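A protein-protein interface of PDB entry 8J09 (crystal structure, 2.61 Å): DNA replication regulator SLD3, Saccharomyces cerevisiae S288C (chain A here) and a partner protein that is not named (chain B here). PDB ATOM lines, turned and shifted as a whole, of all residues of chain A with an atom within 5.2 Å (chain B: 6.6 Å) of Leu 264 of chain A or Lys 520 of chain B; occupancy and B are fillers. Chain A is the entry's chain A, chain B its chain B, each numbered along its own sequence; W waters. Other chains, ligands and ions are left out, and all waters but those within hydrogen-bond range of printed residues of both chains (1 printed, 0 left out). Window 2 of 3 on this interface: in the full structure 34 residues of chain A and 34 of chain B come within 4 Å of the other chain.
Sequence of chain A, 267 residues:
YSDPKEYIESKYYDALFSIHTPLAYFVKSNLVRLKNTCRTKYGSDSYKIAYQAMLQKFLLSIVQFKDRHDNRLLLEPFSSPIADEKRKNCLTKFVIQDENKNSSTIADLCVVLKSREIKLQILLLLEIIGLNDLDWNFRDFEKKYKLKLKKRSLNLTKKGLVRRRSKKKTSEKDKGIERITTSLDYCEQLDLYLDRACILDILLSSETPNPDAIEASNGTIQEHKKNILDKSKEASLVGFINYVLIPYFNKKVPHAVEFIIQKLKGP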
ATOM      1  N   LEU A 194      16.788  -0.735 -14.784  1.00  0.00           N
ATOM      2  CA  LEU A 194      17.361  -1.706 -15.711  1.00  0.00           C
ATOM      3  C   LEU A 194      18.525  -1.103 -16.485  1.00  0.00           C
ATOM      4  O   LEU A 194      19.548  -1.765 -16.699  1.00  0.00           O
ATOM      5  CB  LEU A 194      16.283  -2.218 -16.666  1.00  0.00           C
ATOM      6  CG  LEU A 194      15.176  -3.059 -16.025  1.00  0.00           C
ATOM      7  CD1 LEU A 194      14.015  -3.253 -16.989  1.00  0.00           C
ATOM      8  CD2 LEU A 194      15.725  -4.400 -15.561  1.00  0.00           C
ATOM      9  N   CYS A 198      22.400  -2.442 -16.272  1.00  0.00           N
ATOM     10  CA  CYS A 198      23.205  -2.833 -17.425  1.00  0.00           C
ATOM     11  C   CYS A 198      24.564  -2.145 -17.412  1.00  0.00           C
ATOM     12  O   CYS A 198      25.582  -2.768 -17.736  1.00  0.00           O
ATOM     13  CB  CYS A 198      22.458  -2.519 -18.721  1.00  0.00           C
ATOM     14  SG  CYS A 198      20.969  -3.513 -18.977  1.00  0.00           S
ATOM     15  N   ASP A 201      26.825  -3.991 -15.150  1.00  0.00           N
ATOM     16  CA  ASP A 201      27.299  -5.256 -15.702  1.00  0.00           C
ATOM     17  C   ASP A 201      28.346  -5.033 -16.787  1.00  0.00           C
ATOM     18  O   ASP A 201      29.352  -5.749 -16.839  1.00  0.00           O
ATOM     19  CB  ASP A 201      26.122  -6.059 -16.255  1.00  0.00           C
ATOM     20  CG  ASP A 201      25.551  -7.031 -15.242  1.00  0.00           C
ATOM     21  OD1 ASP A 201      25.671  -6.766 -14.026  1.00  0.00           O
ATOM     22  OD2 ASP A 201      24.986  -8.062 -15.662  1.00  0.00           O
ATOM     23  N   ILE A 202      28.124  -4.050 -17.662  1.00  0.00           N
ATOM     24  CA  ILE A 202      29.046  -3.812 -18.770  1.00  0.00           C
ATOM     25  C   ILE A 202      30.421  -3.411 -18.249  1.00  0.00           C
ATOM     26  O   ILE A 202      31.451  -3.903 -18.726  1.00  0.00           O
ATOM     27  CB  ILE A 202      28.471  -2.748 -19.724  1.00  0.00           C
ATOM     28  CG1 ILE A 202      27.201  -3.263 -20.400  1.00  0.00           C
ATOM     29  CG2 ILE A 202      29.500  -2.351 -20.768  1.00  0.00           C
ATOM     30  CD1 ILE A 202      26.310  -2.164 -20.935  1.00  0.00           C
ATOM     31  N   LEU A 237      22.168 -11.088 -13.594  1.00  0.00           N
ATOM     32  CA  LEU A 237      20.910 -10.697 -14.220  1.00  0.00           C
ATOM     33  C   LEU A 237      20.156 -11.912 -14.746  1.00  0.00           C
ATOM     34  O   LEU A 237      18.938 -12.023 -14.558  1.00  0.00           O
ATOM     35  CB  LEU A 237      21.168  -9.695 -15.346  1.00  0.00           C
ATOM     36  CG  LEU A 237      21.822  -8.368 -14.952  1.00  0.00           C
ATOM     37  CD1 LEU A 237      21.789  -7.386 -16.113  1.00  0.00           C
ATOM     38  CD2 LEU A 237      21.151  -7.771 -13.721  1.00  0.00           C
ATOM     39  N   ILE A 241      16.645 -13.338 -13.210  1.00  0.00           N
ATOM     40  CA  ILE A 241      15.455 -13.577 -14.022  1.00  0.00           C
ATOM     41  C   ILE A 241      14.907 -14.975 -13.761  1.00  0.00           C
ATOM     42  O   ILE A 241      13.726 -15.148 -13.439  1.00  0.00           O
ATOM     43  CB  ILE A 241      15.773 -13.371 -15.513  1.00  0.00           C
ATOM     44  CG1 ILE A 241      15.990 -11.888 -15.821  1.00  0.00           C
ATOM     45  CG2 ILE A 241      14.661 -13.941 -16.381  1.00  0.00           C
ATOM     46  CD1 ILE A 241      16.532 -11.631 -17.211  1.00  0.00           C
ATOM     47  N   PHE A 259       9.261  -7.737 -20.553  1.00  0.00           N
ATOM     48  CA  PHE A 259       9.947  -6.481 -20.841  1.00  0.00           C
ATOM     49  C   PHE A 259      11.344  -6.465 -20.231  1.00  0.00           C
ATOM     50  O   PHE A 259      12.310  -6.051 -20.883  1.00  0.00           O
ATOM     51  CB  PHE A 259       9.113  -5.306 -20.325  1.00  0.00           C
ATOM     52  CG  PHE A 259       9.856  -4.001 -20.284  1.00  0.00           C
ATOM     53  CD1 PHE A 259      10.024  -3.248 -21.436  1.00  0.00           C
ATOM     54  CD2 PHE A 259      10.375  -3.519 -19.093  1.00  0.00           C
ATOM     55  CE1 PHE A 259      10.703  -2.043 -21.401  1.00  0.00           C
ATOM     56  CE2 PHE A 259      11.055  -2.314 -19.052  1.00  0.00           C
ATOM     57  CZ  PHE A 259      11.219  -1.576 -20.208  1.00  0.00           C
ATOM     58  N   ILE A 260      11.468  -6.912 -18.978  1.00  0.00           N
ATOM     59  CA  ILE A 260      12.778  -6.981 -18.335  1.00  0.00           C
ATOM     60  C   ILE A 260      13.688  -7.940 -19.091  1.00  0.00           C
ATOM     61  O   ILE A 260      14.885  -7.680 -19.266  1.00  0.00           O
ATOM     62  CB  ILE A 260      12.624  -7.388 -16.858  1.00  0.00           C
ATOM     63  CG1 ILE A 260      11.961  -6.264 -16.059  1.00  0.00           C
ATOM     64  CG2 ILE A 260      13.975  -7.749 -16.253  1.00  0.00           C
ATOM     65  CD1 ILE A 260      11.360  -6.726 -14.755  1.00  0.00           C
ATOM     66  N   ILE A 261      13.133  -9.058 -19.560  1.00  0.00           N
ATOM     67  CA  ILE A 261      13.933 -10.033 -20.292  1.00  0.00           C
ATOM     68  C   ILE A 261      14.423  -9.440 -21.608  1.00  0.00           C
ATOM     69  O   ILE A 261      15.613  -9.512 -21.933  1.00  0.00           O
ATOM     70  CB  ILE A 261      13.128 -11.328 -20.509  1.00  0.00           C
ATOM     71  CG1 ILE A 261      13.017 -12.106 -19.195  1.00  0.00           C
ATOM     72  CG2 ILE A 261      13.774 -12.191 -21.577  1.00  0.00           C
ATOM     73  CD1 ILE A 261      11.980 -13.208 -19.221  1.00  0.00           C
ATOM     74  N   GLN A 262      13.520  -8.819 -22.371  1.00  0.00           N
ATOM     75  CA  GLN A 262      13.912  -8.256 -23.659  1.00  0.00           C
ATOM     76  C   GLN A 262      14.987  -7.185 -23.510  1.00  0.00           C
ATOM     77  O   GLN A 262      15.829  -7.023 -24.400  1.00  0.00           O
ATOM     78  CB  GLN A 262      12.690  -7.682 -24.379  1.00  0.00           C
ATOM     79  CG  GLN A 262      11.763  -8.737 -24.955  1.00  0.00           C
ATOM     80  CD  GLN A 262      12.509  -9.817 -25.715  1.00  0.00           C
ATOM     81  OE1 GLN A 262      13.330  -9.527 -26.586  1.00  0.00           O
ATOM     82  NE2 GLN A 262      12.227 -11.073 -25.386  1.00  0.00           N
ATOM     83  N   LYS A 263      14.985  -6.456 -22.393  1.00  0.00           N
ATOM     84  CA  LYS A 263      15.976  -5.404 -22.195  1.00  0.00           C
ATOM     85  C   LYS A 263      17.318  -5.972 -21.748  1.00  0.00           C
ATOM     86  O   LYS A 263      18.368  -5.557 -22.250  1.00  0.00           O
ATOM     87  CB  LYS A 263      15.463  -4.387 -21.176  1.00  0.00           C
ATOM     88  CG  LYS A 263      16.222  -3.075 -21.184  1.00  0.00           C
ATOM     89  CD  LYS A 263      15.282  -1.895 -21.023  1.00  0.00           C
ATOM     90  CE  LYS A 263      16.047  -0.641 -20.641  1.00  0.00           C
ATOM     91  NZ  LYS A 263      17.181  -0.381 -21.567  1.00  0.00           N
ATOM     92  N   LEU A 264      17.304  -6.921 -20.808  1.00  0.00           N
ATOM     93  CA  LEU A 264      18.558  -7.466 -20.296  1.00  0.00           C
ATOM     94  C   LEU A 264      19.203  -8.418 -21.297  1.00  0.00           C
ATOM     95  O   LEU A 264      20.430  -8.428 -21.446  1.00  0.00           O
ATOM     96  CB  LEU A 264      18.320  -8.167 -18.959  1.00  0.00           C
ATOM     97  CG  LEU A 264      17.847  -7.285 -17.798  1.00  0.00           C
ATOM     98  CD1 LEU A 264      18.087  -7.973 -16.465  1.00  0.00           C
ATOM     99  CD2 LEU A 264      18.529  -5.926 -17.827  1.00  0.00           C
ATOM    100  N   LYS A 265      18.400  -9.231 -21.990  1.00  0.00           N
ATOM    101  CA  LYS A 265      18.962 -10.110 -23.011  1.00  0.00           C
ATOM    102  C   LYS A 265      19.495  -9.308 -24.191  1.00  0.00           C
ATOM    103  O   LYS A 265      20.555  -9.631 -24.741  1.00  0.00           O
ATOM    104  CB  LYS A 265      17.915 -11.120 -23.487  1.00  0.00           C
ATOM    105  CG  LYS A 265      17.294 -11.971 -22.388  1.00  0.00           C
ATOM    106  CD  LYS A 265      18.318 -12.775 -21.611  1.00  0.00           C
ATOM    107  CE  LYS A 265      17.896 -14.234 -21.523  1.00  0.00           C
ATOM    108  NZ  LYS A 265      17.617 -14.648 -20.121  1.00  0.00           N
ATOM    109  N   GLY A 266      18.780  -8.261 -24.595  1.00  0.00           N
ATOM    110  CA  GLY A 266      19.197  -7.429 -25.699  1.00  0.00           C
ATOM    111  C   GLY A 266      18.790  -8.002 -27.040  1.00  0.00           C
ATOM    112  O   GLY A 266      18.627  -9.217 -27.202  1.00  0.00           O
ATOM    113  N   LYS B 517      29.532  -8.813 -29.775  1.00  0.00           N
ATOM    114  CA  LYS B 517      28.269  -8.258 -29.287  1.00  0.00           C
ATOM    115  C   LYS B 517      28.497  -7.313 -28.108  1.00  0.00           C
ATOM    116  O   LYS B 517      27.900  -7.450 -27.039  1.00  0.00           O
ATOM    117  CB  LYS B 517      27.287  -9.372 -28.919  1.00  0.00           C
ATOM    118  CG  LYS B 517      26.781 -10.166 -30.115  1.00  0.00           C
ATOM    119  CD  LYS B 517      26.067  -9.263 -31.109  1.00  0.00           C
ATOM    120  CE  LYS B 517      25.964  -9.916 -32.478  1.00  0.00           C
ATOM    121  NZ  LYS B 517      25.413  -8.982 -33.501  1.00  0.00           N
ATOM    122  N   LEU B 518      29.379  -6.334 -28.319  1.00  0.00           N
ATOM    123  CA  LEU B 518      29.740  -5.415 -27.246  1.00  0.00           C
ATOM    124  C   LEU B 518      28.736  -4.281 -27.092  1.00  0.00           C
ATOM    125  O   LEU B 518      28.490  -3.828 -25.969  1.00  0.00           O
ATOM    126  CB  LEU B 518      31.138  -4.843 -27.491  1.00  0.00           C
ATOM    127  CG  LEU B 518      32.302  -5.835 -27.441  1.00  0.00           C
ATOM    128  CD1 LEU B 518      33.611  -5.109 -27.180  1.00  0.00           C
ATOM    129  CD2 LEU B 518      32.061  -6.906 -26.386  1.00  0.00           C
ATOM    130  N   ILE B 519      28.151  -3.811 -28.191  1.00  0.00           N
ATOM    131  CA  ILE B 519      27.201  -2.705 -28.127  1.00  0.00           C
ATOM    132  C   ILE B 519      25.956  -3.187 -27.391  1.00  0.00           C
ATOM    133  O   ILE B 519      25.210  -4.029 -27.898  1.00  0.00           O
ATOM    134  CB  ILE B 519      26.849  -2.176 -29.522  1.00  0.00           C
ATOM    135  CG1 ILE B 519      28.115  -1.841 -30.311  1.00  0.00           C
ATOM    136  CG2 ILE B 519      25.949  -0.952 -29.409  1.00  0.00           C
ATOM    137  CD1 ILE B 519      27.865  -1.603 -31.784  1.00  0.00           C
ATOM    138  N   LYS B 520      25.736  -2.667 -26.188  1.00  0.00           N
ATOM    139  CA  LYS B 520      24.499  -2.897 -25.461  1.00  0.00           C
ATOM    140  C   LYS B 520      23.653  -1.632 -25.492  1.00  0.00           C
ATOM    141  O   LYS B 520      24.124  -0.551 -25.857  1.00  0.00           O
ATOM    142  CB  LYS B 520      24.769  -3.349 -24.023  1.00  0.00           C
ATOM    143  CG  LYS B 520      24.710  -4.859 -23.871  1.00  0.00           C
ATOM    144  CD  LYS B 520      24.879  -5.288 -22.428  1.00  0.00           C
ATOM    145  CE  LYS B 520      23.549  -5.686 -21.807  1.00  0.00           C
ATOM    146  NZ  LYS B 520      23.746  -6.491 -20.568  1.00  0.00           N
ATOM    147  N   HIS B 521      22.386  -1.785 -25.111  1.00  0.00           N
ATOM    148  CA  HIS B 521      21.327  -0.894 -25.573  1.00  0.00           C
ATOM    149  C   HIS B 521      20.524  -0.360 -24.395  1.00  0.00           C
ATOM    150  O   HIS B 521      19.814  -1.114 -23.722  1.00  0.00           O
ATOM    151  CB  HIS B 521      20.422  -1.619 -26.575  1.00  0.00           C
ATOM    152  CG  HIS B 521      21.161  -2.188 -27.747  1.00  0.00           C
ATOM    153  ND1 HIS B 521      21.779  -1.397 -28.690  1.00  0.00           N
ATOM    154  CD2 HIS B 521      21.371  -3.469 -28.136  1.00  0.00           C
ATOM    155  CE1 HIS B 521      22.358  -2.164 -29.597  1.00  0.00           C
ATOM    156  NE2 HIS B 521      22.123  -3.426 -29.285  1.00  0.00           N
ATOM    157  N   LEU B 522      20.625   0.943 -24.164  1.00  0.00           N
ATOM    158  CA  LEU B 522      19.881   1.624 -23.122  1.00  0.00           C
ATOM    159  C   LEU B 522      18.718   2.389 -23.755  1.00  0.00           C
ATOM    160  O   LEU B 522      18.514   2.363 -24.971  1.00  0.00           O
ATOM    161  CB  LEU B 522      20.809   2.542 -22.322  1.00  0.00           C
ATOM    162  CG  LEU B 522      21.762   1.888 -21.311  1.00  0.00           C
ATOM    163  CD1 LEU B 522      22.828   1.022 -21.974  1.00  0.00           C
ATOM    164  CD2 LEU B 522      22.422   2.951 -20.458  1.00  0.00           C
ATOM    165  N   TYR B 525      20.310   5.817 -25.472  1.00  0.00           N
ATOM    166  CA  TYR B 525      21.562   5.727 -26.209  1.00  0.00           C
ATOM    167  C   TYR B 525      22.086   4.300 -26.156  1.00  0.00           C
ATOM    168  O   TYR B 525      21.689   3.500 -25.305  1.00  0.00           O
ATOM    169  CB  TYR B 525      22.614   6.710 -25.670  1.00  0.00           C
ATOM    170  CG  TYR B 525      23.146   6.393 -24.286  1.00  0.00           C
ATOM    171  CD1 TYR B 525      24.274   5.600 -24.115  1.00  0.00           C
ATOM    172  CD2 TYR B 525      22.532   6.909 -23.151  1.00  0.00           C
ATOM    173  CE1 TYR B 525      24.767   5.318 -22.857  1.00  0.00           C
ATOM    174  CE2 TYR B 525      23.020   6.632 -21.886  1.00  0.00           C
ATOM    175  CZ  TYR B 525      24.136   5.837 -21.746  1.00  0.00           C
ATOM    176  OH  TYR B 525      24.625   5.557 -20.491  1.00  0.00           O
ATOM    177  N   ARG B 526      22.985   3.997 -27.085  1.00  0.00           N
ATOM    178  CA  ARG B 526      23.683   2.722 -27.120  1.00  0.00           C
ATOM    179  C   ARG B 526      25.090   2.894 -26.570  1.00  0.00           C
ATOM    180  O   ARG B 526      25.754   3.902 -26.830  1.00  0.00           O
ATOM    181  CB  ARG B 526      23.737   2.171 -28.541  1.00  0.00           C
ATOM    182  CG  ARG B 526      22.372   1.957 -29.141  1.00  0.00           C
ATOM    183  CD  ARG B 526      22.502   1.577 -30.587  1.00  0.00           C
ATOM    184  NE  ARG B 526      22.799   2.737 -31.416  1.00  0.00           N
ATOM    185  CZ  ARG B 526      23.054   2.668 -32.718  1.00  0.00           C
ATOM    186  NH1 ARG B 526      23.049   1.492 -33.325  1.00  0.00           N
ATOM    187  NH2 ARG B 526      23.313   3.768 -33.411  1.00  0.00           N
ATOM    188  N   LEU B 527      25.538   1.906 -25.803  1.00  0.00           N
ATOM    189  CA  LEU B 527      26.812   1.973 -25.105  1.00  0.00           C
ATOM    190  C   LEU B 527      27.771   0.945 -25.686  1.00  0.00           C
ATOM    191  O   LEU B 527      27.388  -0.206 -25.920  1.00  0.00           O
ATOM    192  CB  LEU B 527      26.621   1.736 -23.604  1.00  0.00           C
ATOM    193  CG  LEU B 527      27.881   1.710 -22.741  1.00  0.00           C
ATOM    194  CD1 LEU B 527      28.690   2.985 -22.928  1.00  0.00           C
ATOM    195  CD2 LEU B 527      27.512   1.513 -21.279  1.00  0.00           C
ATOM    196  N   CYS B 528      29.012   1.367 -25.918  1.00  0.00           N
ATOM    197  CA  CYS B 528      30.059   0.488 -26.431  1.00  0.00           C
ATOM    198  C   CYS B 528      31.337   0.786 -25.659  1.00  0.00           C
ATOM    199  O   CYS B 528      31.964   1.828 -25.871  1.00  0.00           O
ATOM    200  CB  CYS B 528      30.266   0.687 -27.932  1.00  0.00           C
ATOM    201  SG  CYS B 528      31.540  -0.370 -28.647  1.00  0.00           S
ATOM    202  N   GLU B 558      21.106  -4.136 -36.259  1.00  0.00           N
ATOM    203  CA  GLU B 558      20.456  -3.545 -35.086  1.00  0.00           C
ATOM    204  C   GLU B 558      19.053  -3.036 -35.416  1.00  0.00           C
ATOM    205  O   GLU B 558      18.618  -1.981 -34.942  1.00  0.00           O
ATOM    206  CB  GLU B 558      21.313  -2.445 -34.467  1.00  0.00           C
ATOM    207  CG  GLU B 558      22.021  -2.884 -33.184  1.00  0.00           C
ATOM    208  CD  GLU B 558      23.068  -1.892 -32.713  1.00  0.00           C
ATOM    209  OE1 GLU B 558      24.118  -2.332 -32.196  1.00  0.00           O
ATOM    210  OE2 GLU B 558      22.843  -0.672 -32.853  1.00  0.00           O
ATOM    211  N   LYS B 562      16.194   0.979 -33.369  1.00  0.00           N
ATOM    212  CA  LYS B 562      17.396   1.043 -32.545  1.00  0.00           C
ATOM    213  C   LYS B 562      18.551   1.843 -33.134  1.00  0.00           C
ATOM    214  O   LYS B 562      19.313   2.464 -32.388  1.00  0.00           O
ATOM    215  CB  LYS B 562      17.861  -0.382 -32.249  1.00  0.00           C
ATOM    216  CG  LYS B 562      19.145  -0.476 -31.488  1.00  0.00           C
ATOM    217  CD  LYS B 562      19.111  -1.771 -30.740  1.00  0.00           C
ATOM    218  CE  LYS B 562      18.348  -1.568 -29.456  1.00  0.00           C
ATOM    219  NZ  LYS B 562      18.659  -0.211 -28.932  1.00  0.00           N
HETATM  220  O   HOH W   1      18.377  -3.373 -24.237  1.00  0.00           O
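The backbone carbonyl oxygen of His 521 of chain B lies within hydrogen-bond range of the side-chain amino group of Lys 263 of chain A.
The backbone carbonyl oxygen (O) of Ile 519 of chain B sits at hydrogen-bond distance from a ring nitrogen (NE2) of His 521 of chain B, at 3.4 Å.
The backbone NH (N) of Leu 527 of chain B is in hydrogen-bond range of the backbone carbonyl oxygen (O) of Lys 520 of chain B (2.8 Å).
A ring nitrogen (ND1) of His 521 of chain B sits close to the side-chain amino group (NZ) of Lys 562 of chain B, at 3.3 Å.
Among the printed residues, pairs that only touch across the chains: Ile 202 of chain A with Lys 520 of chain B (3.6 Å), Ile 202 of chain A with Leu 527 of chain B (3.9 Å), Lys 263 of chain A with Leu 522 of chain B (3.7 Å) and Leu 264 of chain A with Lys 520 of chain B (3.9 Å).
Cys 198 of chain A touches none of the printed residues of chain B.
Printed residues of chain B within 4 Å of Ile 202 of chain A: Lys 520 and Leu 527.
Ile 241 of chain A touches none of the printed residues of chain B.
Leu 264 of chain A touches just one residue of chain B: Lys 520.
Lys 520 of chain B touches just these residues of chain A: Ile 202 and Leu 264.
Printed residues of chain A within 4 Å of His 521 of chain B: Lys 263.
The nearest printed residue of chain B that does not touch Leu 264 of chain A is His 521 of chain B (7.0 Å).
Hydrophobic or aromatic side chains of chain A within 4 Å of the printed part of chain B: Ile 202.
Of the 12 printed residues of chain B, 4 touch a printed residue of chain A.
Hydrophobic or aromatic side chains of chain B within 4 Å of the printed part of chain A: Leu 527.
Among the printed residues, 5 pairs touch across the chains.
Water W1 bridges the backbone carbonyl oxygen of His 521 of chain B and the backbone carbonyl oxygen of Lys 263 of chain A.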
